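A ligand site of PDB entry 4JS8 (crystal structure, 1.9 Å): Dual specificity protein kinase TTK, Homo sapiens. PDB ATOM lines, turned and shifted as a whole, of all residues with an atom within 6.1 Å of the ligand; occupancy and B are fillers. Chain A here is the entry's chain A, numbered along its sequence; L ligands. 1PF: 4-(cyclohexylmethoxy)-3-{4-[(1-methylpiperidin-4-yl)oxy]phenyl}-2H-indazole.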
ATOM      1  N   LYS A  15      -0.830  26.592  -2.182  1.00  0.00           N
ATOM      2  CA  LYS A  15      -0.977  26.302  -3.608  1.00  0.00           C
ATOM      3  C   LYS A  15      -1.981  25.173  -3.864  1.00  0.00           C
ATOM      4  O   LYS A  15      -2.201  24.332  -2.979  1.00  0.00           O
ATOM      5  CB  LYS A  15       0.387  25.942  -4.255  1.00  0.00           C
ATOM      6  CG  LYS A  15       1.080  24.701  -3.688  1.00  0.00           C
ATOM      7  CD  LYS A  15       2.410  24.392  -4.387  1.00  0.00           C
ATOM      8  CE  LYS A  15       2.249  23.594  -5.665  1.00  0.00           C
ATOM      9  NZ  LYS A  15       3.569  23.247  -6.256  1.00  0.00           N
ATOM     10  N   ILE A  17      -2.637  21.760  -5.506  1.00  0.00           N
ATOM     11  CA  ILE A  17      -1.789  20.655  -5.935  1.00  0.00           C
ATOM     12  C   ILE A  17      -2.555  19.648  -6.811  1.00  0.00           C
ATOM     13  O   ILE A  17      -1.937  18.902  -7.564  1.00  0.00           O
ATOM     14  CB  ILE A  17      -1.090  19.982  -4.722  1.00  0.00           C
ATOM     15  CG1 ILE A  17      -2.102  19.531  -3.638  1.00  0.00           C
ATOM     16  CG2 ILE A  17      -0.024  20.935  -4.142  1.00  0.00           C
ATOM     17  CD1 ILE A  17      -1.512  18.706  -2.488  1.00  0.00           C
ATOM     18  N   GLY A  18      -3.892  19.676  -6.750  1.00  0.00           N
ATOM     19  CA  GLY A  18      -4.741  18.789  -7.540  1.00  0.00           C
ATOM     20  C   GLY A  18      -6.113  19.353  -7.843  1.00  0.00           C
ATOM     21  O   GLY A  18      -6.639  20.182  -7.098  1.00  0.00           O
ATOM     22  N   VAL A  25      -7.620  19.882  -4.452  1.00  0.00           N
ATOM     23  CA  VAL A  25      -6.768  19.593  -3.287  1.00  0.00           C
ATOM     24  C   VAL A  25      -5.783  20.755  -3.131  1.00  0.00           C
ATOM     25  O   VAL A  25      -5.099  21.126  -4.096  1.00  0.00           O
ATOM     26  CB  VAL A  25      -6.069  18.204  -3.314  1.00  0.00           C
ATOM     27  CG1 VAL A  25      -5.205  17.997  -2.065  1.00  0.00           C
ATOM     28  CG2 VAL A  25      -7.096  17.077  -3.402  1.00  0.00           C
ATOM     29  N   GLN A  27      -2.641  22.677  -0.675  1.00  0.00           N
ATOM     30  CA  GLN A  27      -1.584  22.625   0.344  1.00  0.00           C
ATOM     31  C   GLN A  27      -1.884  23.808   1.257  1.00  0.00           C
ATOM     32  O   GLN A  27      -1.988  24.929   0.760  1.00  0.00           O
ATOM     33  CB  GLN A  27      -0.219  22.712  -0.334  1.00  0.00           C
ATOM     34  CG  GLN A  27       0.914  22.099   0.468  1.00  0.00           C
ATOM     35  CD  GLN A  27       2.181  22.009  -0.333  1.00  0.00           C
ATOM     36  OE1 GLN A  27       2.786  23.011  -0.728  1.00  0.00           O
ATOM     37  NE2 GLN A  27       2.637  20.788  -0.600  1.00  0.00           N
ATOM     38  N   ALA A  37      -3.165  19.072   3.928  1.00  0.00           N
ATOM     39  CA  ALA A  37      -3.748  19.040   2.589  1.00  0.00           C
ATOM     40  C   ALA A  37      -5.250  19.050   2.755  1.00  0.00           C
ATOM     41  O   ALA A  37      -5.780  18.277   3.553  1.00  0.00           O
ATOM     42  CB  ALA A  37      -3.271  17.812   1.822  1.00  0.00           C
ATOM     43  N   LYS A  39      -8.917  18.759   0.809  1.00  0.00           N
ATOM     44  CA  LYS A  39      -9.677  18.410  -0.373  1.00  0.00           C
ATOM     45  C   LYS A  39     -11.025  19.107  -0.299  1.00  0.00           C
ATOM     46  O   LYS A  39     -11.747  18.951   0.697  1.00  0.00           O
ATOM     47  CB  LYS A  39      -9.829  16.887  -0.531  1.00  0.00           C
ATOM     48  CG  LYS A  39     -10.537  16.478  -1.829  1.00  0.00           C
ATOM     49  CD  LYS A  39     -10.666  14.974  -1.964  1.00  0.00           C
ATOM     50  CE  LYS A  39     -11.416  14.613  -3.226  1.00  0.00           C
ATOM     51  NZ  LYS A  39     -11.315  13.164  -3.540  1.00  0.00           N
ATOM     52  N   ILE A  72      -3.505   7.357   4.401  1.00  0.00           N
ATOM     53  CA  ILE A  72      -3.456   8.808   4.659  1.00  0.00           C
ATOM     54  C   ILE A  72      -4.317   9.157   5.894  1.00  0.00           C
ATOM     55  O   ILE A  72      -5.406   8.615   6.075  1.00  0.00           O
ATOM     56  CB  ILE A  72      -3.865   9.640   3.405  1.00  0.00           C
ATOM     57  CG1 ILE A  72      -3.614  11.153   3.612  1.00  0.00           C
ATOM     58  CG2 ILE A  72      -5.305   9.383   2.937  1.00  0.00           C
ATOM     59  CD1 ILE A  72      -2.692  11.723   2.694  1.00  0.00           C
ATOM     60  N   MET A  88      -6.528  16.627   5.658  1.00  0.00           N
ATOM     61  CA  MET A  88      -5.667  15.443   5.630  1.00  0.00           C
ATOM     62  C   MET A  88      -4.206  15.792   5.830  1.00  0.00           C
ATOM     63  O   MET A  88      -3.834  16.962   5.719  1.00  0.00           O
ATOM     64  CB  MET A  88      -5.846  14.685   4.301  1.00  0.00           C
ATOM     65  CG  MET A  88      -7.197  14.005   4.174  1.00  0.00           C
ATOM     66  SD  MET A  88      -7.551  13.414   2.512  1.00  0.00           S
ATOM     67  CE  MET A  88      -7.940  14.905   1.726  1.00  0.00           C
ATOM     68  N   GLU A  89      -3.371  14.767   6.124  1.00  0.00           N
ATOM     69  CA  GLU A  89      -1.928  14.975   6.280  1.00  0.00           C
ATOM     70  C   GLU A  89      -1.348  15.306   4.893  1.00  0.00           C
ATOM     71  O   GLU A  89      -1.847  14.806   3.883  1.00  0.00           O
ATOM     72  CB  GLU A  89      -1.229  13.771   6.939  1.00  0.00           C
ATOM     73  CG  GLU A  89      -1.039  12.536   6.075  1.00  0.00           C
ATOM     74  CD  GLU A  89      -0.384  11.359   6.761  1.00  0.00           C
ATOM     75  OE1 GLU A  89       0.773  11.480   7.210  1.00  0.00           O
ATOM     76  OE2 GLU A  89      -1.029  10.278   6.820  1.00  0.00           O
ATOM     77  N   CYS A  90      -0.366  16.209   4.862  1.00  0.00           N
ATOM     78  CA  CYS A  90       0.267  16.614   3.602  1.00  0.00           C
ATOM     79  C   CYS A  90       1.558  15.856   3.411  1.00  0.00           C
ATOM     80  O   CYS A  90       2.401  15.811   4.310  1.00  0.00           O
ATOM     81  CB  CYS A  90       0.502  18.132   3.587  1.00  0.00           C
ATOM     82  SG  CYS A  90       1.084  18.766   1.997  1.00  0.00           S
ATOM     83  N   GLY A  91       1.710  15.249   2.247  1.00  0.00           N
ATOM     84  CA  GLY A  91       2.919  14.511   1.898  1.00  0.00           C
ATOM     85  C   GLY A  91       3.900  15.366   1.132  1.00  0.00           C
ATOM     86  O   GLY A  91       3.584  16.487   0.737  1.00  0.00           O
ATOM     87  N   ASN A  92       5.109  14.822   0.908  1.00  0.00           N
ATOM     88  CA  ASN A  92       6.162  15.518   0.175  1.00  0.00           C
ATOM     89  C   ASN A  92       5.883  15.490  -1.327  1.00  0.00           C
ATOM     90  O   ASN A  92       5.874  16.537  -1.977  1.00  0.00           O
ATOM     91  CB  ASN A  92       7.528  14.910   0.487  1.00  0.00           C
ATOM     92  CG  ASN A  92       7.943  15.044   1.933  1.00  0.00           C
ATOM     93  OD1 ASN A  92       7.471  14.312   2.798  1.00  0.00           O
ATOM     94  ND2 ASN A  92       8.831  15.985   2.205  1.00  0.00           N
ATOM     95  N   ILE A  93       5.632  14.282  -1.868  1.00  0.00           N
ATOM     96  CA  ILE A  93       5.371  14.055  -3.293  1.00  0.00           C
ATOM     97  C   ILE A  93       4.621  12.716  -3.491  1.00  0.00           C
ATOM     98  O   ILE A  93       4.818  11.786  -2.701  1.00  0.00           O
ATOM     99  CB  ILE A  93       6.737  14.078  -4.073  1.00  0.00           C
ATOM    100  CG1 ILE A  93       6.542  14.154  -5.615  1.00  0.00           C
ATOM    101  CG2 ILE A  93       7.709  12.951  -3.638  1.00  0.00           C
ATOM    102  CD1 ILE A  93       7.754  14.702  -6.407  1.00  0.00           C
ATOM    103  N   ASP A  94       3.791  12.620  -4.543  1.00  0.00           N
ATOM    104  CA  ASP A  94       3.110  11.382  -4.913  1.00  0.00           C
ATOM    105  C   ASP A  94       4.124  10.491  -5.634  1.00  0.00           C
ATOM    106  O   ASP A  94       5.090  11.004  -6.208  1.00  0.00           O
ATOM    107  CB  ASP A  94       1.878  11.659  -5.782  1.00  0.00           C
ATOM    108  CG  ASP A  94       2.206  12.343  -7.093  1.00  0.00           C
ATOM    109  OD1 ASP A  94       2.598  13.524  -7.061  1.00  0.00           O
ATOM    110  OD2 ASP A  94       2.028  11.706  -8.148  1.00  0.00           O
ATOM    111  N   SER A  97       4.847  11.337  -9.608  1.00  0.00           N
ATOM    112  CA  SER A  97       5.726  12.494  -9.854  1.00  0.00           C
ATOM    113  C   SER A  97       7.168  12.189  -9.449  1.00  0.00           C
ATOM    114  O   SER A  97       8.102  12.702 -10.066  1.00  0.00           O
ATOM    115  CB  SER A  97       5.223  13.717  -9.099  1.00  0.00           C
ATOM    116  OG  SER A  97       3.880  14.035  -9.425  1.00  0.00           O
ATOM    117  N   ALA A 137       0.016   7.377  -8.617  1.00  0.00           N
ATOM    118  CA  ALA A 137      -0.634   8.615  -8.176  1.00  0.00           C
ATOM    119  C   ALA A 137      -1.522   8.404  -6.926  1.00  0.00           C
ATOM    120  O   ALA A 137      -1.817   9.374  -6.238  1.00  0.00           O
ATOM    121  CB  ALA A 137      -1.456   9.206  -9.302  1.00  0.00           C
ATOM    122  N   ASN A 138      -1.934   7.138  -6.639  1.00  0.00           N
ATOM    123  CA  ASN A 138      -2.752   6.768  -5.486  1.00  0.00           C
ATOM    124  C   ASN A 138      -1.904   6.594  -4.218  1.00  0.00           C
ATOM    125  O   ASN A 138      -2.462   6.370  -3.139  1.00  0.00           O
ATOM    126  CB  ASN A 138      -3.535   5.481  -5.756  1.00  0.00           C
ATOM    127  CG  ASN A 138      -4.515   5.564  -6.898  1.00  0.00           C
ATOM    128  OD1 ASN A 138      -4.462   4.764  -7.835  1.00  0.00           O
ATOM    129  ND2 ASN A 138      -5.446   6.503  -6.831  1.00  0.00           N
ATOM    130  N   LEU A 140       1.379   8.183  -1.786  1.00  0.00           N
ATOM    131  CA  LEU A 140       2.040   9.402  -1.318  1.00  0.00           C
ATOM    132  C   LEU A 140       3.289   9.107  -0.508  1.00  0.00           C
ATOM    133  O   LEU A 140       3.255   8.217   0.343  1.00  0.00           O
ATOM    134  CB  LEU A 140       1.054  10.139  -0.407  1.00  0.00           C
ATOM    135  CG  LEU A 140       0.774  11.627  -0.580  1.00  0.00           C
ATOM    136  CD1 LEU A 140       0.261  12.175   0.701  1.00  0.00           C
ATOM    137  CD2 LEU A 140       2.013  12.424  -0.962  1.00  0.00           C
ATOM    138  N   ILE A 149      -3.580   7.016  -0.655  1.00  0.00           N
ATOM    139  CA  ILE A 149      -4.351   8.261  -0.637  1.00  0.00           C
ATOM    140  C   ILE A 149      -5.859   7.982  -0.709  1.00  0.00           C
ATOM    141  O   ILE A 149      -6.607   8.558   0.079  1.00  0.00           O
ATOM    142  CB  ILE A 149      -3.884   9.203  -1.799  1.00  0.00           C
ATOM    143  CG1 ILE A 149      -2.377   9.517  -1.706  1.00  0.00           C
ATOM    144  CG2 ILE A 149      -4.699  10.482  -1.854  1.00  0.00           C
ATOM    145  CD1 ILE A 149      -1.745  10.081  -2.992  1.00  0.00           C
ATOM    146  N   MET A 157      -8.287  12.321  -9.400  1.00  0.00           N
ATOM    147  CA  MET A 157      -7.866  13.711  -9.653  1.00  0.00           C
ATOM    148  C   MET A 157      -6.509  13.804 -10.341  1.00  0.00           C
ATOM    149  O   MET A 157      -5.614  12.994 -10.057  1.00  0.00           O
ATOM    150  CB  MET A 157      -7.837  14.497  -8.337  1.00  0.00           C
ATOM    151  CG  MET A 157      -9.210  14.697  -7.714  1.00  0.00           C
ATOM    152  SD  MET A 157      -9.157  15.516  -6.104  1.00  0.00           S
ATOM    153  CE  MET A 157      -8.726  17.111  -6.592  1.00  0.00           C
ATOM    154  N   GLN A 158      -6.339  14.822 -11.217  1.00  0.00           N
ATOM    155  CA  GLN A 158      -5.093  15.067 -11.963  1.00  0.00           C
ATOM    156  C   GLN A 158      -4.206  16.128 -11.246  1.00  0.00           C
ATOM    157  O   GLN A 158      -4.735  17.000 -10.562  1.00  0.00           O
ATOM    158  CB  GLN A 158      -5.383  15.476 -13.426  1.00  0.00           C
ATOM    159  CG  GLN A 158      -6.203  16.748 -13.633  1.00  0.00           C
ATOM    160  CD  GLN A 158      -6.243  17.172 -15.084  1.00  0.00           C
ATOM    161  OE1 GLN A 158      -5.655  18.185 -15.480  1.00  0.00           O
ATOM    162  NE2 GLN A 158      -6.949  16.421 -15.917  1.00  0.00           N
ATOM    163  N   PRO A 159      -2.858  16.051 -11.407  1.00  0.00           N
ATOM    164  CA  PRO A 159      -1.976  16.996 -10.703  1.00  0.00           C
ATOM    165  C   PRO A 159      -2.014  18.447 -11.207  1.00  0.00           C
ATOM    166  O   PRO A 159      -2.534  18.737 -12.292  1.00  0.00           O
ATOM    167  CB  PRO A 159      -0.579  16.410 -10.921  1.00  0.00           C
ATOM    168  CG  PRO A 159      -0.687  15.622 -12.164  1.00  0.00           C
ATOM    169  CD  PRO A 159      -2.065  15.044 -12.151  1.00  0.00           C
ATOM    170  N   ASP A 160      -1.455  19.355 -10.383  1.00  0.00           N
ATOM    171  CA  ASP A 160      -1.304  20.792 -10.639  1.00  0.00           C
ATOM    172  C   ASP A 160      -0.002  21.295 -10.008  1.00  0.00           C
ATOM    173  O   ASP A 160       0.291  20.981  -8.853  1.00  0.00           O
ATOM    174  CB  ASP A 160      -2.507  21.596 -10.107  1.00  0.00           C
ATOM    175  CG  ASP A 160      -3.796  21.385 -10.882  1.00  0.00           C
ATOM    176  OD1 ASP A 160      -3.789  21.579 -12.122  1.00  0.00           O
ATOM    177  OD2 ASP A 160      -4.818  21.085 -10.248  1.00  0.00           O
ATOM    178  N   TPO A 161       0.787  22.061 -10.773  1.00  0.00           N
ATOM    179  CA  TPO A 161       2.061  22.609 -10.314  1.00  0.00           C
ATOM    180  CB  TPO A 161       3.149  21.499 -10.290  1.00  0.00           C
ATOM    181  CG2 TPO A 161       3.322  20.898 -11.694  1.00  0.00           C
ATOM    182  OG1 TPO A 161       4.412  22.031  -9.842  1.00  0.00           O
ATOM    183  P   TPO A 161       5.216  21.041  -8.988  1.00  0.00           P
ATOM    184  O1P TPO A 161       6.658  21.523  -8.937  1.00  0.00           O
ATOM    185  O2P TPO A 161       4.665  20.990  -7.573  1.00  0.00           O
ATOM    186  O3P TPO A 161       5.255  19.631  -9.568  1.00  0.00           O
ATOM    187  C   TPO A 161       2.517  23.785 -11.170  1.00  0.00           C
ATOM    188  O   TPO A 161       1.690  24.567 -11.650  1.00  0.00           O
HETATM  189  C10 1PF L   1      -0.073  15.429  -1.768  1.00  0.00           C
HETATM  190  C14 1PF L   1      -2.960  14.570   0.242  1.00  0.00           C
HETATM  191  C15 1PF L   1      -4.337  14.179   0.460  1.00  0.00           C
HETATM  192  C16 1PF L   1      -5.181  13.950  -0.616  1.00  0.00           C
HETATM  193  C17 1PF L   1      -4.689  14.140  -1.923  1.00  0.00           C
HETATM  194  C20 1PF L   1      -3.637  14.304  -4.657  1.00  0.00           C
HETATM  195  C22 1PF L   1      -1.993  15.568  -6.087  1.00  0.00           C
HETATM  196  C23 1PF L   1      -1.140  15.620  -7.324  1.00  0.00           C
HETATM  197  C24 1PF L   1      -0.615  14.278  -7.818  1.00  0.00           C
HETATM  198  C31 1PF L   1       1.925  17.874  -6.805  1.00  0.00           C
HETATM  199  C30 1PF L   1       2.282  18.329  -5.427  1.00  0.00           C
HETATM  200  C28 1PF L   1       0.961  16.275  -1.394  1.00  0.00           C
HETATM  201  C26 1PF L   1      -2.301  13.078  -6.390  1.00  0.00           C
HETATM  202  C25 1PF L   1      -1.577  13.126  -7.710  1.00  0.00           C
HETATM  203  C18 1PF L   1      -3.331  14.520  -2.153  1.00  0.00           C
HETATM  204  C01 1PF L   1       2.795  17.394  -9.167  1.00  0.00           C
HETATM  205  N02 1PF L   1       3.075  17.739  -7.728  1.00  0.00           N
HETATM  206  C03 1PF L   1       4.282  17.141  -7.140  1.00  0.00           C
HETATM  207  C04 1PF L   1       4.593  17.551  -5.707  1.00  0.00           C
HETATM  208  C05 1PF L   1       3.411  17.578  -4.829  1.00  0.00           C
HETATM  209  O06 1PF L   1       3.085  16.250  -4.486  1.00  0.00           O
HETATM  210  C07 1PF L   1       2.040  16.002  -3.562  1.00  0.00           C
HETATM  211  C08 1PF L   1       1.030  15.102  -3.925  1.00  0.00           C
HETATM  212  C09 1PF L   1      -0.009  14.805  -3.041  1.00  0.00           C
HETATM  213  C11 1PF L   1      -1.063  15.141  -0.809  1.00  0.00           C
HETATM  214  N12 1PF L   1      -0.841  15.187   0.498  1.00  0.00           N
HETATM  215  N13 1PF L   1      -1.988  14.811   1.159  1.00  0.00           N
HETATM  216  O19 1PF L   1      -2.874  14.675  -3.474  1.00  0.00           O
HETATM  217  C21 1PF L   1      -2.962  14.415  -6.049  1.00  0.00           C
HETATM  218  C27 1PF L   1      -2.440  14.751  -1.043  1.00  0.00           C
HETATM  219  C29 1PF L   1       2.021  16.569  -2.266  1.00  0.00           C
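O3P of TPO 161 lies close to a nitrogen (N02) of the ligand (3.4 Å). A nitrogen (N12) of the ligand lies close to the backbone NH (N) of Gly 91 (3.1 Å). The backbone carbonyl oxygen (O) of Glu 89 sits close to a nitrogen (N13) of the ligand, at 2.7 Å.
The backbone carbonyl oxygen of Gly 18 is in hydrogen-bond range of the backbone NH of Val 25 (2.8 Å). The side-chain sulfur (SG) of Cys 90 sits at hydrogen-bond distance from the side-chain amide nitrogen (NE2) of Gln 27 (3.6 Å). N of Met 88 is in hydrogen-bond range of O of Ala 37, 2.8 Å away. O of Ile 17 sits at hydrogen-bond distance from N of Asp 160. O2P of TPO 161 lies within salt-bridge range of the side-chain amino group of Lys 15. The backbone carbonyl oxygen (O) of Asn 138 sits at hydrogen-bond distance from the backbone NH (N) of Ile 149, at 2.8 Å. N of Ile 17 sits at hydrogen-bond distance from O of Val 25. OG of Ser 97 is in hydrogen-bond range of OD1 of Asp 94, 2.7 Å away.
O of Ile 17 touches C23 of the ligand, 3.4 Å away. Val 25 touches the ligand (CG1 to C17, 3.9 Å). Ala 37 touches the ligand. CD1 of Ile 72 touches N13 of the ligand (3.5 Å). CE of Met 88 touches C16 of the ligand (3.7 Å). CA of Cys 90 touches N12 of the ligand, at 3.6 Å. Asn 92 touches the ligand. CA of Ile 93 touches O06 of the ligand, 3.4 Å away. Asp 94 touches the ligand (OD1 to C24, 3.4 Å). Ser 97 touches the ligand (OG to C01, 3.5 Å). O of Ala 137 touches C26 of the ligand (3.7 Å). Leu 140 touches the ligand. Ile 149 touches the ligand (CG2 to C17, 3.7 Å). CB of Pro 159 touches C23 of the ligand (3.7 Å). Hydrophobic or aromatic side chains within 4 Å of the ligand: Ile 17, Val 25, Ala 37, Ile 72, Met 88, Ile 93, Leu 140, Ile 149 and Pro 159. Within 4 Å of the ligand: Ile 17, Val 25, Ala 37, Ile 72, Met 88, Glu 89, Cys 90, Gly 91, Asn 92, Ile 93, Asp 94, Ser 97, Ala 137, Leu 140, Ile 149, Pro 159 and TPO 161. Along chain A the residues within 4 Å of the ligand span positions 17 to 161.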
